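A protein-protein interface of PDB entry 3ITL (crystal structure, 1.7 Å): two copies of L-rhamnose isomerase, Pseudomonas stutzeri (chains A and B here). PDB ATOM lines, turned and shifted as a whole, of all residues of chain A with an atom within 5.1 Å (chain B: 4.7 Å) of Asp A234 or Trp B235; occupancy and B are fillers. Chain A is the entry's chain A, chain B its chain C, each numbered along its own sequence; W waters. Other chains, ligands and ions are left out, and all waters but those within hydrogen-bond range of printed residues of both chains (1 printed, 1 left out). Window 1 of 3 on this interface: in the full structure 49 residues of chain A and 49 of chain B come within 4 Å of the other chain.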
ATOM      1  N   HIS A 220     -27.741 -11.461 -28.151  1.00  0.00           N
ATOM      2  CA  HIS A 220     -26.464 -10.785 -28.337  1.00  0.00           C
ATOM      3  C   HIS A 220     -25.668 -11.374 -29.493  1.00  0.00           C
ATOM      4  O   HIS A 220     -25.875 -12.521 -29.890  1.00  0.00           O
ATOM      5  CB  HIS A 220     -25.614 -10.848 -27.061  1.00  0.00           C
ATOM      6  CG  HIS A 220     -25.308 -12.240 -26.597  1.00  0.00           C
ATOM      7  ND1 HIS A 220     -26.142 -12.948 -25.759  1.00  0.00           N
ATOM      8  CD2 HIS A 220     -24.256 -13.055 -26.854  1.00  0.00           C
ATOM      9  CE1 HIS A 220     -25.619 -14.136 -25.517  1.00  0.00           C
ATOM     10  NE2 HIS A 220     -24.474 -14.227 -26.170  1.00  0.00           N
ATOM     11  N   LYS A 221     -24.760 -10.567 -30.034  1.00  0.00           N
ATOM     12  CA  LYS A 221     -23.892 -10.987 -31.129  1.00  0.00           C
ATOM     13  C   LYS A 221     -22.672 -10.072 -31.104  1.00  0.00           C
ATOM     14  O   LYS A 221     -22.810  -8.853 -31.086  1.00  0.00           O
ATOM     15  CB  LYS A 221     -24.610 -10.870 -32.471  1.00  0.00           C
ATOM     16  CG  LYS A 221     -23.834 -11.516 -33.614  1.00  0.00           C
ATOM     17  CD  LYS A 221     -24.633 -11.511 -34.905  1.00  0.00           C
ATOM     18  CE  LYS A 221     -23.852 -12.193 -36.023  1.00  0.00           C
ATOM     19  NZ  LYS A 221     -24.532 -12.057 -37.340  1.00  0.00           N
ATOM     20  N   VAL A 232     -25.897  -4.772 -28.606  1.00  0.00           N
ATOM     21  CA  VAL A 232     -26.080  -5.971 -27.790  1.00  0.00           C
ATOM     22  C   VAL A 232     -24.969  -6.908 -28.258  1.00  0.00           C
ATOM     23  O   VAL A 232     -25.207  -7.850 -29.009  1.00  0.00           O
ATOM     24  CB  VAL A 232     -27.458  -6.614 -28.033  1.00  0.00           C
ATOM     25  CG1 VAL A 232     -27.727  -7.680 -26.978  1.00  0.00           C
ATOM     26  CG2 VAL A 232     -28.546  -5.544 -27.987  1.00  0.00           C
ATOM     27  N   GLN A 233     -23.754  -6.630 -27.796  1.00  0.00           N
ATOM     28  CA  GLN A 233     -22.572  -7.383 -28.215  1.00  0.00           C
ATOM     29  C   GLN A 233     -22.268  -8.703 -27.523  1.00  0.00           C
ATOM     30  O   GLN A 233     -21.702  -9.603 -28.145  1.00  0.00           O
ATOM     31  CB  GLN A 233     -21.331  -6.476 -28.151  1.00  0.00           C
ATOM     32  CG  GLN A 233     -20.441  -6.656 -26.915  1.00  0.00           C
ATOM     33  CD  GLN A 233     -21.023  -6.026 -25.668  1.00  0.00           C
ATOM     34  OE1 GLN A 233     -22.241  -5.950 -25.510  1.00  0.00           O
ATOM     35  NE2 GLN A 233     -20.151  -5.585 -24.761  1.00  0.00           N
ATOM     36  N   ASP A 234     -22.609  -8.826 -26.245  1.00  0.00           N
ATOM     37  CA  ASP A 234     -22.345 -10.077 -25.540  1.00  0.00           C
ATOM     38  C   ASP A 234     -23.374 -10.360 -24.451  1.00  0.00           C
ATOM     39  O   ASP A 234     -24.310  -9.581 -24.256  1.00  0.00           O
ATOM     40  CB  ASP A 234     -20.923 -10.094 -24.953  1.00  0.00           C
ATOM     41  CG  ASP A 234     -20.697  -9.022 -23.905  1.00  0.00           C
ATOM     42  OD1 ASP A 234     -21.679  -8.535 -23.314  1.00  0.00           O
ATOM     43  OD2 ASP A 234     -19.521  -8.678 -23.657  1.00  0.00           O
ATOM     44  N   TRP A 235     -23.200 -11.476 -23.745  1.00  0.00           N
ATOM     45  CA  TRP A 235     -24.151 -11.864 -22.708  1.00  0.00           C
ATOM     46  C   TRP A 235     -24.193 -10.933 -21.498  1.00  0.00           C
ATOM     47  O   TRP A 235     -25.176 -10.925 -20.756  1.00  0.00           O
ATOM     48  CB  TRP A 235     -23.891 -13.302 -22.243  1.00  0.00           C
ATOM     49  CG  TRP A 235     -22.790 -13.456 -21.235  1.00  0.00           C
ATOM     50  CD1 TRP A 235     -21.446 -13.507 -21.478  1.00  0.00           C
ATOM     51  CD2 TRP A 235     -22.947 -13.581 -19.816  1.00  0.00           C
ATOM     52  NE1 TRP A 235     -20.754 -13.655 -20.295  1.00  0.00           N
ATOM     53  CE2 TRP A 235     -21.653 -13.704 -19.260  1.00  0.00           C
ATOM     54  CE3 TRP A 235     -24.058 -13.599 -18.959  1.00  0.00           C
ATOM     55  CZ2 TRP A 235     -21.437 -13.843 -17.886  1.00  0.00           C
ATOM     56  CZ3 TRP A 235     -23.843 -13.736 -17.588  1.00  0.00           C
ATOM     57  CH2 TRP A 235     -22.540 -13.856 -17.068  1.00  0.00           C
ATOM     58  N   GLY A 236     -23.130 -10.164 -21.289  1.00  0.00           N
ATOM     59  CA  GLY A 236     -23.112  -9.234 -20.173  1.00  0.00           C
ATOM     60  C   GLY A 236     -24.120  -8.129 -20.437  1.00  0.00           C
ATOM     61  O   GLY A 236     -24.922  -7.765 -19.575  1.00  0.00           O
ATOM     62  N   THR A 237     -24.083  -7.585 -21.648  1.00  0.00           N
ATOM     63  CA  THR A 237     -25.019  -6.535 -22.014  1.00  0.00           C
ATOM     64  C   THR A 237     -26.407  -7.141 -22.062  1.00  0.00           C
ATOM     65  O   THR A 237     -27.384  -6.511 -21.667  1.00  0.00           O
ATOM     66  CB  THR A 237     -24.687  -5.942 -23.393  1.00  0.00           C
ATOM     67  OG1 THR A 237     -23.452  -5.223 -23.311  1.00  0.00           O
ATOM     68  CG2 THR A 237     -25.793  -5.004 -23.860  1.00  0.00           C
ATOM     69  N   ASN A 238     -26.486  -8.378 -22.543  1.00  0.00           N
ATOM     70  CA  ASN A 238     -27.766  -9.059 -22.653  1.00  0.00           C
ATOM     71  C   ASN A 238     -28.391  -9.242 -21.277  1.00  0.00           C
ATOM     72  O   ASN A 238     -29.599  -9.057 -21.106  1.00  0.00           O
ATOM     73  CB  ASN A 238     -27.601 -10.413 -23.349  1.00  0.00           C
ATOM     74  CG  ASN A 238     -28.825 -10.791 -24.172  1.00  0.00           C
ATOM     75  OD1 ASN A 238     -29.820 -10.065 -24.176  1.00  0.00           O
ATOM     76  ND2 ASN A 238     -28.758 -11.918 -24.870  1.00  0.00           N
ATOM     77  N   LEU A 240     -27.884  -7.360 -18.676  1.00  0.00           N
ATOM     78  CA  LEU A 240     -28.320  -6.036 -18.239  1.00  0.00           C
ATOM     79  C   LEU A 240     -29.673  -5.682 -18.849  1.00  0.00           C
ATOM     80  O   LEU A 240     -30.514  -5.059 -18.198  1.00  0.00           O
ATOM     81  CB  LEU A 240     -27.283  -4.969 -18.619  1.00  0.00           C
ATOM     82  CG  LEU A 240     -25.934  -5.047 -17.900  1.00  0.00           C
ATOM     83  CD1 LEU A 240     -24.960  -4.065 -18.526  1.00  0.00           C
ATOM     84  CD2 LEU A 240     -26.122  -4.752 -16.413  1.00  0.00           C
ATOM     85  N   HIS B 220     -11.815  -9.948 -13.510  1.00  0.00           N
ATOM     86  CA  HIS B 220     -12.090 -11.074 -14.392  1.00  0.00           C
ATOM     87  C   HIS B 220     -10.901 -11.396 -15.292  1.00  0.00           C
ATOM     88  O   HIS B 220     -10.044 -10.549 -15.548  1.00  0.00           O
ATOM     89  CB  HIS B 220     -13.328 -10.803 -15.261  1.00  0.00           C
ATOM     90  CG  HIS B 220     -13.216  -9.585 -16.124  1.00  0.00           C
ATOM     91  ND1 HIS B 220     -13.578  -8.328 -15.690  1.00  0.00           N
ATOM     92  CD2 HIS B 220     -12.781  -9.433 -17.397  1.00  0.00           C
ATOM     93  CE1 HIS B 220     -13.372  -7.454 -16.658  1.00  0.00           C
ATOM     94  NE2 HIS B 220     -12.889  -8.098 -17.706  1.00  0.00           N
ATOM     95  N   ASP B 234     -15.260 -13.297 -17.232  1.00  0.00           N
ATOM     96  CA  ASP B 234     -15.439 -12.082 -18.023  1.00  0.00           C
ATOM     97  C   ASP B 234     -16.150 -10.961 -17.271  1.00  0.00           C
ATOM     98  O   ASP B 234     -16.490 -11.112 -16.091  1.00  0.00           O
ATOM     99  CB  ASP B 234     -16.151 -12.382 -19.356  1.00  0.00           C
ATOM    100  CG  ASP B 234     -17.551 -12.942 -19.181  1.00  0.00           C
ATOM    101  OD1 ASP B 234     -18.166 -12.743 -18.118  1.00  0.00           O
ATOM    102  OD2 ASP B 234     -18.049 -13.577 -20.138  1.00  0.00           O
ATOM    103  N   TRP B 235     -16.360  -9.835 -17.948  1.00  0.00           N
ATOM    104  CA  TRP B 235     -16.997  -8.689 -17.307  1.00  0.00           C
ATOM    105  C   TRP B 235     -18.458  -8.925 -16.937  1.00  0.00           C
ATOM    106  O   TRP B 235     -19.001  -8.230 -16.078  1.00  0.00           O
ATOM    107  CB  TRP B 235     -16.867  -7.437 -18.180  1.00  0.00           C
ATOM    108  CG  TRP B 235     -17.879  -7.325 -19.271  1.00  0.00           C
ATOM    109  CD1 TRP B 235     -17.849  -7.938 -20.488  1.00  0.00           C
ATOM    110  CD2 TRP B 235     -19.087  -6.561 -19.233  1.00  0.00           C
ATOM    111  NE1 TRP B 235     -18.967  -7.601 -21.216  1.00  0.00           N
ATOM    112  CE2 TRP B 235     -19.745  -6.757 -20.468  1.00  0.00           C
ATOM    113  CE3 TRP B 235     -19.679  -5.728 -18.274  1.00  0.00           C
ATOM    114  CZ2 TRP B 235     -20.970  -6.149 -20.771  1.00  0.00           C
ATOM    115  CZ3 TRP B 235     -20.898  -5.123 -18.574  1.00  0.00           C
ATOM    116  CH2 TRP B 235     -21.529  -5.338 -19.814  1.00  0.00           C
ATOM    117  N   GLY B 236     -19.089  -9.900 -17.582  1.00  0.00           N
ATOM    118  CA  GLY B 236     -20.471 -10.218 -17.275  1.00  0.00           C
ATOM    119  C   GLY B 236     -20.550 -10.838 -15.891  1.00  0.00           C
ATOM    120  O   GLY B 236     -21.353 -10.414 -15.054  1.00  0.00           O
ATOM    121  N   THR B 237     -19.723 -11.849 -15.647  1.00  0.00           N
ATOM    122  CA  THR B 237     -19.695 -12.496 -14.337  1.00  0.00           C
ATOM    123  C   THR B 237     -19.232 -11.470 -13.303  1.00  0.00           C
ATOM    124  O   THR B 237     -19.738 -11.427 -12.177  1.00  0.00           O
ATOM    125  CB  THR B 237     -18.723 -13.699 -14.307  1.00  0.00           C
ATOM    126  OG1 THR B 237     -19.258 -14.774 -15.092  1.00  0.00           O
ATOM    127  CG2 THR B 237     -18.521 -14.189 -12.878  1.00  0.00           C
ATOM    128  N   ASN B 238     -18.273 -10.635 -13.692  1.00  0.00           N
ATOM    129  CA  ASN B 238     -17.749  -9.619 -12.791  1.00  0.00           C
ATOM    130  C   ASN B 238     -18.860  -8.662 -12.373  1.00  0.00           C
ATOM    131  O   ASN B 238     -18.950  -8.273 -11.207  1.00  0.00           O
ATOM    132  CB  ASN B 238     -16.606  -8.845 -13.462  1.00  0.00           C
ATOM    133  CG  ASN B 238     -15.585  -8.329 -12.456  1.00  0.00           C
ATOM    134  OD1 ASN B 238     -15.791  -8.422 -11.243  1.00  0.00           O
ATOM    135  ND2 ASN B 238     -14.483  -7.780 -12.955  1.00  0.00           N
ATOM    136  N   TYR B 239     -19.716  -8.283 -13.318  1.00  0.00           N
ATOM    137  CA  TYR B 239     -20.812  -7.388 -12.980  1.00  0.00           C
ATOM    138  C   TYR B 239     -21.744  -8.058 -11.976  1.00  0.00           C
ATOM    139  O   TYR B 239     -22.172  -7.428 -11.012  1.00  0.00           O
ATOM    140  CB  TYR B 239     -21.620  -6.993 -14.214  1.00  0.00           C
ATOM    141  CG  TYR B 239     -22.800  -6.131 -13.842  1.00  0.00           C
ATOM    142  CD1 TYR B 239     -22.621  -4.799 -13.480  1.00  0.00           C
ATOM    143  CD2 TYR B 239     -24.084  -6.672 -13.761  1.00  0.00           C
ATOM    144  CE1 TYR B 239     -23.688  -4.024 -13.038  1.00  0.00           C
ATOM    145  CE2 TYR B 239     -25.161  -5.906 -13.318  1.00  0.00           C
ATOM    146  CZ  TYR B 239     -24.954  -4.586 -12.957  1.00  0.00           C
ATOM    147  OH  TYR B 239     -26.006  -3.826 -12.499  1.00  0.00           O
ATOM    148  N   ILE B 267     -16.793  -2.357 -22.912  1.00  0.00           N
ATOM    149  CA  ILE B 267     -16.960  -2.919 -21.575  1.00  0.00           C
ATOM    150  C   ILE B 267     -16.785  -1.800 -20.551  1.00  0.00           C
ATOM    151  O   ILE B 267     -17.545  -1.694 -19.593  1.00  0.00           O
ATOM    152  CB  ILE B 267     -15.931  -4.033 -21.309  1.00  0.00           C
ATOM    153  CG1 ILE B 267     -16.276  -5.263 -22.157  1.00  0.00           C
ATOM    154  CG2 ILE B 267     -15.916  -4.385 -19.833  1.00  0.00           C
ATOM    155  CD1 ILE B 267     -15.234  -6.373 -22.096  1.00  0.00           C
ATOM    156  N   ARG B 270     -19.890   0.333 -20.480  1.00  0.00           N
ATOM    157  CA  ARG B 270     -20.983  -0.367 -19.813  1.00  0.00           C
ATOM    158  C   ARG B 270     -20.820  -0.325 -18.294  1.00  0.00           C
ATOM    159  O   ARG B 270     -21.780  -0.065 -17.567  1.00  0.00           O
ATOM    160  CB  ARG B 270     -21.042  -1.822 -20.292  1.00  0.00           C
ATOM    161  CG  ARG B 270     -21.462  -1.988 -21.757  1.00  0.00           C
ATOM    162  CD  ARG B 270     -22.974  -1.904 -21.935  1.00  0.00           C
ATOM    163  NE  ARG B 270     -23.384  -2.158 -23.318  1.00  0.00           N
ATOM    164  CZ  ARG B 270     -23.414  -1.237 -24.278  1.00  0.00           C
ATOM    165  NH1 ARG B 270     -23.061   0.017 -24.019  1.00  0.00           N
ATOM    166  NH2 ARG B 270     -23.806  -1.568 -25.502  1.00  0.00           N
ATOM    167  N   LEU B 271     -19.604  -0.577 -17.809  1.00  0.00           N
ATOM    168  CA  LEU B 271     -19.363  -0.553 -16.370  1.00  0.00           C
ATOM    169  C   LEU B 271     -19.570   0.849 -15.800  1.00  0.00           C
ATOM    170  O   LEU B 271     -20.058   1.003 -14.681  1.00  0.00           O
ATOM    171  CB  LEU B 271     -17.949  -1.046 -16.054  1.00  0.00           C
ATOM    172  CG  LEU B 271     -17.737  -2.548 -16.279  1.00  0.00           C
ATOM    173  CD1 LEU B 271     -16.281  -2.899 -16.061  1.00  0.00           C
ATOM    174  CD2 LEU B 271     -18.632  -3.343 -15.336  1.00  0.00           C
HETATM  175  O   HOH W   1     -18.203 -11.338 -22.454  1.00  0.00           O
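Among the printed residues, merely in contact across the chains: Trp A235 with Gly B236 (3.7 Å), Trp A235 with Thr B237 (3.5 Å), Gly A236 with Trp B235 (3.7 Å), Thr A237 with Trp B235 (3.5 Å), Leu A240 with Trp B235 (3.9 Å) and Leu A240 with Tyr B239 (3.4 Å).
Of the printed residues of chain A, Asp B234 touches Trp A235.
Of chain A, only Asp A234, Gly A236, Thr A237 and Leu A240 come within 4 Å of Trp B235.
Of the printed residues of chain A, Tyr B239 touches Leu A240 (3.4 Å).
Of the 10 printed residues of chain B, 6 touch a printed residue of chain A.
Hydrophobic or aromatic side chains of chain B that line the printed part of chain A: Trp B235 and Tyr B239.
Hydrophobic or aromatic side chains of chain A that line the printed part of chain B: Trp A235 and Leu A240.
The side-chain carboxylate of Asp A234 lies within hydrogen-bond range of the side-chain amide nitrogen of Gln A233 (3.3 Å).
OE1 of Gln A233 sits at hydrogen-bond distance from OG1 of Thr A237, 2.6 Å away.
The side-chain carboxylate (OD1) of Asp A234 lies within hydrogen-bond range of the backbone NH (N) of Thr A237, at 3.1 Å.
The side-chain carboxylate of Asp B234 is in hydrogen-bond range of the backbone NH of Thr B237 (3.1 Å).
N of Gly B236 is in hydrogen-bond range of OD1 of Asp B234 (3.0 Å).
The side-chain carboxylate of Asp A234 is in hydrogen-bond range of the backbone NH of Gly A236 (3.0 Å).
Asp A234 touches Trp B235, and with the chains exchanged Trp A235 touches Asp B234.
Trp A235 touches Gly B236, and with the chains exchanged Gly A236 touches Trp B235.
Trp A235 touches Thr B237, and with the chains exchanged Thr A237 touches Trp B235.
Positions printed for both chains: 220, 234, 235, 236, 237 and 238.
The indole nitrogen (NE1) of Trp A235 lies within hydrogen-bond range of the side-chain carboxylate (OD2) of Asp B234 (2.7 Å).
The side-chain hydroxyl (OG1) of Thr A237 lies within hydrogen-bond range of the guanidinium group (NE) of Arg B270 (3.1 Å).
The indole nitrogen (NE1) of Trp B235 sits at hydrogen-bond distance from the side-chain carboxylate (OD2) of Asp A234 (2.7 Å).
Water W1 bridges the side-chain carboxylate of Asp A234 (3.2 Å) and the side-chain carboxylate of Asp B234 (3.2 Å).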
